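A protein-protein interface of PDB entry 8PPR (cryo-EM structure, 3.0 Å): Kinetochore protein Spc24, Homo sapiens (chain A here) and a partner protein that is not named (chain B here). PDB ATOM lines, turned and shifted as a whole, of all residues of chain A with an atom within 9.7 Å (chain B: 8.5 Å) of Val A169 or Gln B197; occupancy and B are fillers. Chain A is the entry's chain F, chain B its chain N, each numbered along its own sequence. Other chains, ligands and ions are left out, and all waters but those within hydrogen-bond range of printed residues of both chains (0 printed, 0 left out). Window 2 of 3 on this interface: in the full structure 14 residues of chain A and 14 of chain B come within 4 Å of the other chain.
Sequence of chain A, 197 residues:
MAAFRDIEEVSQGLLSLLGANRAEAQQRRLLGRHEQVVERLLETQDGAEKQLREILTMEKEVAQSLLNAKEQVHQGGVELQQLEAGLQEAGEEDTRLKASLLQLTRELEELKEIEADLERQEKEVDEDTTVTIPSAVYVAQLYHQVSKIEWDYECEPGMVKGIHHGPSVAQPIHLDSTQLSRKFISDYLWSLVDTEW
Of the 14 printed residues of chain A, 5 touch a printed residue of chain B.
Printed residues of chain A that touch a printed residue of chain B: Ile A163, Val A169, Ala A170, Gln A171 and Pro A172.
Hydrophobic or aromatic side chains of chain A within 4 Å of the printed part of chain B: Ile A163, Val A169 and Pro A172.
Of the 15 printed residues of chain B, 4 touch a printed residue of chain A.
Printed residues of chain B that touch a printed residue of chain A: Gln B197, Gly B200, Phe B201 and Val B204.
Among the printed residues, pairs that only touch across the chains: Ile A163 with Val B204 (3.6 Å), Val A169 with Gln B197 (3.3 Å), Val A169 with Phe B201 (3.5 Å), Ala A170 with Phe B201 (3.3 Å), Ala A170 with Val B204 (3.7 Å), Gln A171 with Val B204 (3.4 Å), Pro A172 with Gly B200 (3.3 Å) and Pro A172 with Val B204 (3.2 Å).
The backbone carbonyl oxygen (O) of Gln A171 is in hydrogen-bond range of the backbone NH (N) of His A164, 2.9 Å away.
Val A169 touches two residues of chain B.
Of chain A, only Val A169 (3.3 Å) comes within 4 Å of Gln B197.
No residue of chain B comes within 4 Å of Ser A168.
Of chain B, only Phe B201 (3.3 Å) and Val B204 (3.7 Å) come within 4 Å of Ala A170.
No residue of chain A comes within 4 Å of Gly B198.
Of chain A, only Pro A172 comes within 4 Å of Gly B200.
Of the printed residues of chain B, Ile A163 touches Val B204.
Printed residues of chain B within 4 Å of Pro A172: Gly B200 (3.3 Å) and Val B204 (3.2 Å).
Of the printed residues of chain A, Val B204 touches Ile A163, Ala A170, Gln A171 and Pro A172.
Printed residues of chain A within 4 Å of Phe B201: Val A169 and Ala A170.
Asp A194 touches none of the printed residues of chain B.
His A165 touches none of the printed residues of chain B.
The nearest residue of chain A that does not touch Gln B197 is Ala A170 (5.3 Å).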
ATOM      1  N   LYS A 148      23.600 -35.767 -15.890  1.00  0.00           N
ATOM      2  CA  LYS A 148      24.446 -34.574 -15.826  1.00  0.00           C
ATOM      3  C   LYS A 148      23.722 -33.436 -15.113  1.00  0.00           C
ATOM      4  O   LYS A 148      23.840 -32.266 -15.480  1.00  0.00           O
ATOM      5  CB  LYS A 148      24.911 -34.142 -17.218  1.00  0.00           C
ATOM      6  CG  LYS A 148      25.689 -35.209 -17.963  1.00  0.00           C
ATOM      7  CD  LYS A 148      26.112 -34.719 -19.334  1.00  0.00           C
ATOM      8  CE  LYS A 148      27.302 -33.781 -19.235  1.00  0.00           C
ATOM      9  NZ  LYS A 148      28.526 -34.490 -18.771  1.00  0.00           N
ATOM     10  N   ILE A 163      21.405 -27.610 -11.565  1.00  0.00           N
ATOM     11  CA  ILE A 163      22.257 -27.226 -12.682  1.00  0.00           C
ATOM     12  C   ILE A 163      22.251 -28.351 -13.704  1.00  0.00           C
ATOM     13  O   ILE A 163      22.472 -29.516 -13.353  1.00  0.00           O
ATOM     14  CB  ILE A 163      23.694 -26.924 -12.220  1.00  0.00           C
ATOM     15  CG1 ILE A 163      23.708 -25.720 -11.275  1.00  0.00           C
ATOM     16  CG2 ILE A 163      24.604 -26.713 -13.417  1.00  0.00           C
ATOM     17  CD1 ILE A 163      25.017 -25.537 -10.542  1.00  0.00           C
ATOM     18  N   HIS A 164      22.004 -28.004 -14.962  1.00  0.00           N
ATOM     19  CA  HIS A 164      22.023 -28.963 -16.056  1.00  0.00           C
ATOM     20  C   HIS A 164      23.297 -28.774 -16.865  1.00  0.00           C
ATOM     21  O   HIS A 164      23.539 -27.692 -17.409  1.00  0.00           O
ATOM     22  CB  HIS A 164      20.793 -28.803 -16.948  1.00  0.00           C
ATOM     23  CG  HIS A 164      20.357 -30.075 -17.603  1.00  0.00           C
ATOM     24  ND1 HIS A 164      21.239 -30.922 -18.238  1.00  0.00           N
ATOM     25  CD2 HIS A 164      19.139 -30.654 -17.706  1.00  0.00           C
ATOM     26  CE1 HIS A 164      20.580 -31.962 -18.716  1.00  0.00           C
ATOM     27  NE2 HIS A 164      19.304 -31.826 -18.405  1.00  0.00           N
ATOM     28  N   HIS A 165      24.110 -29.826 -16.938  1.00  0.00           N
ATOM     29  CA  HIS A 165      25.337 -29.818 -17.717  1.00  0.00           C
ATOM     30  C   HIS A 165      25.155 -30.438 -19.095  1.00  0.00           C
ATOM     31  O   HIS A 165      26.130 -30.565 -19.843  1.00  0.00           O
ATOM     32  CB  HIS A 165      26.444 -30.544 -16.954  1.00  0.00           C
ATOM     33  CG  HIS A 165      26.851 -29.859 -15.688  1.00  0.00           C
ATOM     34  ND1 HIS A 165      27.924 -28.997 -15.619  1.00  0.00           N
ATOM     35  CD2 HIS A 165      26.322 -29.901 -14.442  1.00  0.00           C
ATOM     36  CE1 HIS A 165      28.043 -28.543 -14.384  1.00  0.00           C
ATOM     37  NE2 HIS A 165      27.082 -29.076 -13.651  1.00  0.00           N
ATOM     38  N   GLY A 166      23.932 -30.828 -19.443  1.00  0.00           N
ATOM     39  CA  GLY A 166      23.638 -31.402 -20.734  1.00  0.00           C
ATOM     40  C   GLY A 166      23.976 -30.491 -21.899  1.00  0.00           C
ATOM     41  O   GLY A 166      24.674 -30.890 -22.835  1.00  0.00           O
ATOM     42  N   PRO A 167      23.485 -29.253 -21.873  1.00  0.00           N
ATOM     43  CA  PRO A 167      23.849 -28.303 -22.927  1.00  0.00           C
ATOM     44  C   PRO A 167      25.332 -27.972 -22.896  1.00  0.00           C
ATOM     45  O   PRO A 167      26.040 -28.229 -21.919  1.00  0.00           O
ATOM     46  CB  PRO A 167      23.001 -27.068 -22.604  1.00  0.00           C
ATOM     47  CG  PRO A 167      21.854 -27.598 -21.829  1.00  0.00           C
ATOM     48  CD  PRO A 167      22.405 -28.728 -21.020  1.00  0.00           C
ATOM     49  N   SER A 168      25.801 -27.396 -24.006  1.00  0.00           N
ATOM     50  CA  SER A 168      27.205 -27.013 -24.105  1.00  0.00           C
ATOM     51  C   SER A 168      27.568 -25.991 -23.037  1.00  0.00           C
ATOM     52  O   SER A 168      28.637 -26.076 -22.420  1.00  0.00           O
ATOM     53  CB  SER A 168      27.500 -26.463 -25.499  1.00  0.00           C
ATOM     54  OG  SER A 168      27.001 -27.332 -26.500  1.00  0.00           O
ATOM     55  N   VAL A 169      26.692 -25.020 -22.805  1.00  0.00           N
ATOM     56  CA  VAL A 169      26.836 -24.062 -21.716  1.00  0.00           C
ATOM     57  C   VAL A 169      25.849 -24.457 -20.630  1.00  0.00           C
ATOM     58  O   VAL A 169      24.639 -24.522 -20.876  1.00  0.00           O
ATOM     59  CB  VAL A 169      26.598 -22.621 -22.188  1.00  0.00           C
ATOM     60  CG1 VAL A 169      26.679 -21.663 -21.015  1.00  0.00           C
ATOM     61  CG2 VAL A 169      27.614 -22.244 -23.253  1.00  0.00           C
ATOM     62  N   ALA A 170      26.367 -24.740 -19.437  1.00  0.00           N
ATOM     63  CA  ALA A 170      25.517 -25.176 -18.339  1.00  0.00           C
ATOM     64  C   ALA A 170      24.479 -24.110 -18.009  1.00  0.00           C
ATOM     65  O   ALA A 170      24.778 -22.913 -17.981  1.00  0.00           O
ATOM     66  CB  ALA A 170      26.363 -25.489 -17.105  1.00  0.00           C
ATOM     67  N   GLN A 171      23.254 -24.554 -17.760  1.00  0.00           N
ATOM     68  CA  GLN A 171      22.149 -23.659 -17.470  1.00  0.00           C
ATOM     69  C   GLN A 171      21.466 -24.082 -16.181  1.00  0.00           C
ATOM     70  O   GLN A 171      21.451 -25.269 -15.839  1.00  0.00           O
ATOM     71  CB  GLN A 171      21.131 -23.648 -18.618  1.00  0.00           C
ATOM     72  CG  GLN A 171      20.487 -24.991 -18.886  1.00  0.00           C
ATOM     73  CD  GLN A 171      19.551 -24.950 -20.073  1.00  0.00           C
ATOM     74  OE1 GLN A 171      19.979 -25.062 -21.221  1.00  0.00           O
ATOM     75  NE2 GLN A 171      18.262 -24.783 -19.804  1.00  0.00           N
ATOM     76  N   PRO A 172      20.899 -23.130 -15.440  1.00  0.00           N
ATOM     77  CA  PRO A 172      20.331 -23.461 -14.126  1.00  0.00           C
ATOM     78  C   PRO A 172      18.919 -24.007 -14.267  1.00  0.00           C
ATOM     79  O   PRO A 172      18.071 -23.414 -14.938  1.00  0.00           O
ATOM     80  CB  PRO A 172      20.343 -22.118 -13.390  1.00  0.00           C
ATOM     81  CG  PRO A 172      20.175 -21.112 -14.481  1.00  0.00           C
ATOM     82  CD  PRO A 172      20.810 -21.687 -15.729  1.00  0.00           C
ATOM     83  N   ILE A 173      18.671 -25.146 -13.634  1.00  0.00           N
ATOM     84  CA  ILE A 173      17.339 -25.737 -13.633  1.00  0.00           C
ATOM     85  C   ILE A 173      16.514 -25.056 -12.551  1.00  0.00           C
ATOM     86  O   ILE A 173      16.874 -25.083 -11.370  1.00  0.00           O
ATOM     87  CB  ILE A 173      17.404 -27.252 -13.408  1.00  0.00           C
ATOM     88  CG1 ILE A 173      18.471 -27.866 -14.313  1.00  0.00           C
ATOM     89  CG2 ILE A 173      16.049 -27.882 -13.671  1.00  0.00           C
ATOM     90  CD1 ILE A 173      18.655 -29.340 -14.107  1.00  0.00           C
ATOM     91  N   LEU A 192      17.104 -31.511 -22.499  1.00  0.00           N
ATOM     92  CA  LEU A 192      18.363 -30.805 -22.311  1.00  0.00           C
ATOM     93  C   LEU A 192      19.573 -31.722 -22.398  1.00  0.00           C
ATOM     94  O   LEU A 192      20.696 -31.226 -22.537  1.00  0.00           O
ATOM     95  CB  LEU A 192      18.356 -30.090 -20.962  1.00  0.00           C
ATOM     96  CG  LEU A 192      17.321 -28.979 -20.782  1.00  0.00           C
ATOM     97  CD1 LEU A 192      17.698 -28.090 -19.611  1.00  0.00           C
ATOM     98  CD2 LEU A 192      17.172 -28.163 -22.056  1.00  0.00           C
ATOM     99  N   ASP A 194      22.234 -34.123 -24.077  1.00  0.00           N
ATOM    100  CA  ASP A 194      22.787 -34.238 -25.420  1.00  0.00           C
ATOM    101  C   ASP A 194      22.643 -35.674 -25.909  1.00  0.00           C
ATOM    102  O   ASP A 194      23.149 -36.606 -25.274  1.00  0.00           O
ATOM    103  CB  ASP A 194      24.251 -33.810 -25.431  1.00  0.00           C
ATOM    104  CG  ASP A 194      24.632 -33.078 -26.698  1.00  0.00           C
ATOM    105  OD1 ASP A 194      23.934 -33.257 -27.719  1.00  0.00           O
ATOM    106  OD2 ASP A 194      25.628 -32.324 -26.676  1.00  0.00           O
ATOM    107  N   SER B 190      19.881 -12.425 -32.358  1.00  0.00           N
ATOM    108  CA  SER B 190      20.745 -13.394 -31.699  1.00  0.00           C
ATOM    109  C   SER B 190      21.382 -12.871 -30.421  1.00  0.00           C
ATOM    110  O   SER B 190      21.561 -13.641 -29.470  1.00  0.00           O
ATOM    111  CB  SER B 190      21.851 -13.843 -32.657  1.00  0.00           C
ATOM    112  OG  SER B 190      22.762 -14.710 -32.009  1.00  0.00           O
ATOM    113  N   LEU B 191      21.735 -11.588 -30.377  1.00  0.00           N
ATOM    114  CA  LEU B 191      22.468 -11.060 -29.228  1.00  0.00           C
ATOM    115  C   LEU B 191      21.708 -11.197 -27.914  1.00  0.00           C
ATOM    116  O   LEU B 191      22.324 -11.608 -26.914  1.00  0.00           O
ATOM    117  CB  LEU B 191      22.861  -9.606 -29.505  1.00  0.00           C
ATOM    118  CG  LEU B 191      23.902  -9.002 -28.566  1.00  0.00           C
ATOM    119  CD1 LEU B 191      25.051  -9.972 -28.375  1.00  0.00           C
ATOM    120  CD2 LEU B 191      24.407  -7.685 -29.128  1.00  0.00           C
ATOM    121  N   PRO B 192      20.414 -10.867 -27.823  1.00  0.00           N
ATOM    122  CA  PRO B 192      19.705 -11.096 -26.554  1.00  0.00           C
ATOM    123  C   PRO B 192      19.703 -12.549 -26.123  1.00  0.00           C
ATOM    124  O   PRO B 192      19.744 -12.827 -24.919  1.00  0.00           O
ATOM    125  CB  PRO B 192      18.286 -10.593 -26.852  1.00  0.00           C
ATOM    126  CG  PRO B 192      18.464  -9.612 -27.947  1.00  0.00           C
ATOM    127  CD  PRO B 192      19.551 -10.180 -28.799  1.00  0.00           C
ATOM    128  N   ALA B 193      19.654 -13.488 -27.071  1.00  0.00           N
ATOM    129  CA  ALA B 193      19.705 -14.899 -26.707  1.00  0.00           C
ATOM    130  C   ALA B 193      21.025 -15.246 -26.033  1.00  0.00           C
ATOM    131  O   ALA B 193      21.048 -15.937 -25.008  1.00  0.00           O
ATOM    132  CB  ALA B 193      19.489 -15.767 -27.946  1.00  0.00           C
ATOM    133  N   LEU B 194      22.139 -14.765 -26.591  1.00  0.00           N
ATOM    134  CA  LEU B 194      23.429 -15.009 -25.960  1.00  0.00           C
ATOM    135  C   LEU B 194      23.539 -14.301 -24.620  1.00  0.00           C
ATOM    136  O   LEU B 194      24.154 -14.834 -23.691  1.00  0.00           O
ATOM    137  CB  LEU B 194      24.568 -14.576 -26.880  1.00  0.00           C
ATOM    138  CG  LEU B 194      25.933 -15.063 -26.389  1.00  0.00           C
ATOM    139  CD1 LEU B 194      25.918 -16.569 -26.181  1.00  0.00           C
ATOM    140  CD2 LEU B 194      27.036 -14.666 -27.349  1.00  0.00           C
ATOM    141  N   ILE B 195      22.963 -13.105 -24.500  1.00  0.00           N
ATOM    142  CA  ILE B 195      22.967 -12.416 -23.214  1.00  0.00           C
ATOM    143  C   ILE B 195      22.223 -13.239 -22.171  1.00  0.00           C
ATOM    144  O   ILE B 195      22.680 -13.388 -21.031  1.00  0.00           O
ATOM    145  CB  ILE B 195      22.365 -11.007 -23.365  1.00  0.00           C
ATOM    146  CG1 ILE B 195      23.350 -10.080 -24.076  1.00  0.00           C
ATOM    147  CG2 ILE B 195      21.983 -10.438 -22.009  1.00  0.00           C
ATOM    148  CD1 ILE B 195      22.807  -8.692 -24.319  1.00  0.00           C
ATOM    149  N   GLU B 196      21.071 -13.793 -22.550  1.00  0.00           N
ATOM    150  CA  GLU B 196      20.306 -14.624 -21.628  1.00  0.00           C
ATOM    151  C   GLU B 196      21.079 -15.879 -21.246  1.00  0.00           C
ATOM    152  O   GLU B 196      21.087 -16.284 -20.077  1.00  0.00           O
ATOM    153  CB  GLU B 196      18.964 -14.992 -22.257  1.00  0.00           C
ATOM    154  CG  GLU B 196      17.961 -13.857 -22.252  1.00  0.00           C
ATOM    155  CD  GLU B 196      17.689 -13.326 -20.860  1.00  0.00           C
ATOM    156  OE1 GLU B 196      17.689 -14.127 -19.903  1.00  0.00           O
ATOM    157  OE2 GLU B 196      17.481 -12.102 -20.724  1.00  0.00           O
ATOM    158  N   GLN B 197      21.731 -16.511 -22.224  1.00  0.00           N
ATOM    159  CA  GLN B 197      22.522 -17.701 -21.931  1.00  0.00           C
ATOM    160  C   GLN B 197      23.665 -17.378 -20.979  1.00  0.00           C
ATOM    161  O   GLN B 197      23.938 -18.137 -20.041  1.00  0.00           O
ATOM    162  CB  GLN B 197      23.058 -18.304 -23.227  1.00  0.00           C
ATOM    163  CG  GLN B 197      24.201 -19.280 -23.021  1.00  0.00           C
ATOM    164  CD  GLN B 197      24.501 -20.092 -24.261  1.00  0.00           C
ATOM    165  OE1 GLN B 197      25.632 -20.110 -24.747  1.00  0.00           O
ATOM    166  NE2 GLN B 197      23.487 -20.771 -24.782  1.00  0.00           N
ATOM    167  N   GLY B 198      24.341 -16.250 -21.200  1.00  0.00           N
ATOM    168  CA  GLY B 198      25.414 -15.854 -20.305  1.00  0.00           C
ATOM    169  C   GLY B 198      24.918 -15.547 -18.907  1.00  0.00           C
ATOM    170  O   GLY B 198      25.582 -15.870 -17.919  1.00  0.00           O
ATOM    171  N   GLU B 199      23.749 -14.913 -18.803  1.00  0.00           N
ATOM    172  CA  GLU B 199      23.166 -14.659 -17.491  1.00  0.00           C
ATOM    173  C   GLU B 199      22.860 -15.963 -16.769  1.00  0.00           C
ATOM    174  O   GLU B 199      23.166 -16.112 -15.578  1.00  0.00           O
ATOM    175  CB  GLU B 199      21.900 -13.821 -17.641  1.00  0.00           C
ATOM    176  CG  GLU B 199      22.132 -12.327 -17.575  1.00  0.00           C
ATOM    177  CD  GLU B 199      21.072 -11.550 -18.326  1.00  0.00           C
ATOM    178  OE1 GLU B 199      20.234 -12.186 -18.999  1.00  0.00           O
ATOM    179  OE2 GLU B 199      21.076 -10.303 -18.248  1.00  0.00           O
ATOM    180  N   GLY B 200      22.269 -16.924 -17.480  1.00  0.00           N
ATOM    181  CA  GLY B 200      22.002 -18.218 -16.877  1.00  0.00           C
ATOM    182  C   GLY B 200      23.269 -18.925 -16.443  1.00  0.00           C
ATOM    183  O   GLY B 200      23.309 -19.560 -15.387  1.00  0.00           O
ATOM    184  N   PHE B 201      24.324 -18.825 -17.251  1.00  0.00           N
ATOM    185  CA  PHE B 201      25.583 -19.469 -16.894  1.00  0.00           C
ATOM    186  C   PHE B 201      26.233 -18.806 -15.687  1.00  0.00           C
ATOM    187  O   PHE B 201      26.805 -19.488 -14.831  1.00  0.00           O
ATOM    188  CB  PHE B 201      26.533 -19.460 -18.086  1.00  0.00           C
ATOM    189  CG  PHE B 201      27.793 -20.218 -17.840  1.00  0.00           C
ATOM    190  CD1 PHE B 201      27.763 -21.587 -17.650  1.00  0.00           C
ATOM    191  CD2 PHE B 201      29.009 -19.565 -17.794  1.00  0.00           C
ATOM    192  CE1 PHE B 201      28.921 -22.288 -17.415  1.00  0.00           C
ATOM    193  CE2 PHE B 201      30.172 -20.262 -17.565  1.00  0.00           C
ATOM    194  CZ  PHE B 201      30.129 -21.626 -17.374  1.00  0.00           C
ATOM    195  N   SER B 202      26.162 -17.478 -15.601  1.00  0.00           N
ATOM    196  CA  SER B 202      26.658 -16.794 -14.412  1.00  0.00           C
ATOM    197  C   SER B 202      25.867 -17.215 -13.183  1.00  0.00           C
ATOM    198  O   SER B 202      26.424 -17.367 -12.089  1.00  0.00           O
ATOM    199  CB  SER B 202      26.582 -15.280 -14.607  1.00  0.00           C
ATOM    200  OG  SER B 202      27.319 -14.601 -13.605  1.00  0.00           O
ATOM    201  N   GLN B 203      24.560 -17.400 -13.346  1.00  0.00           N
ATOM    202  CA  GLN B 203      23.732 -17.855 -12.236  1.00  0.00           C
ATOM    203  C   GLN B 203      24.129 -19.270 -11.814  1.00  0.00           C
ATOM    204  O   GLN B 203      24.177 -19.592 -10.619  1.00  0.00           O
ATOM    205  CB  GLN B 203      22.267 -17.774 -12.660  1.00  0.00           C
ATOM    206  CG  GLN B 203      21.264 -17.902 -11.555  1.00  0.00           C
ATOM    207  CD  GLN B 203      19.854 -17.635 -12.032  1.00  0.00           C
ATOM    208  OE1 GLN B 203      19.645 -16.983 -13.056  1.00  0.00           O
ATOM    209  NE2 GLN B 203      18.875 -18.133 -11.289  1.00  0.00           N
ATOM    210  N   VAL B 204      24.441 -20.122 -12.792  1.00  0.00           N
ATOM    211  CA  VAL B 204      24.982 -21.445 -12.494  1.00  0.00           C
ATOM    212  C   VAL B 204      26.264 -21.320 -11.689  1.00  0.00           C
ATOM    213  O   VAL B 204      26.470 -22.030 -10.697  1.00  0.00           O
ATOM    214  CB  VAL B 204      25.227 -22.226 -13.797  1.00  0.00           C
ATOM    215  CG1 VAL B 204      26.078 -23.452 -13.526  1.00  0.00           C
ATOM    216  CG2 VAL B 204      23.926 -22.623 -14.417  1.00  0.00           C
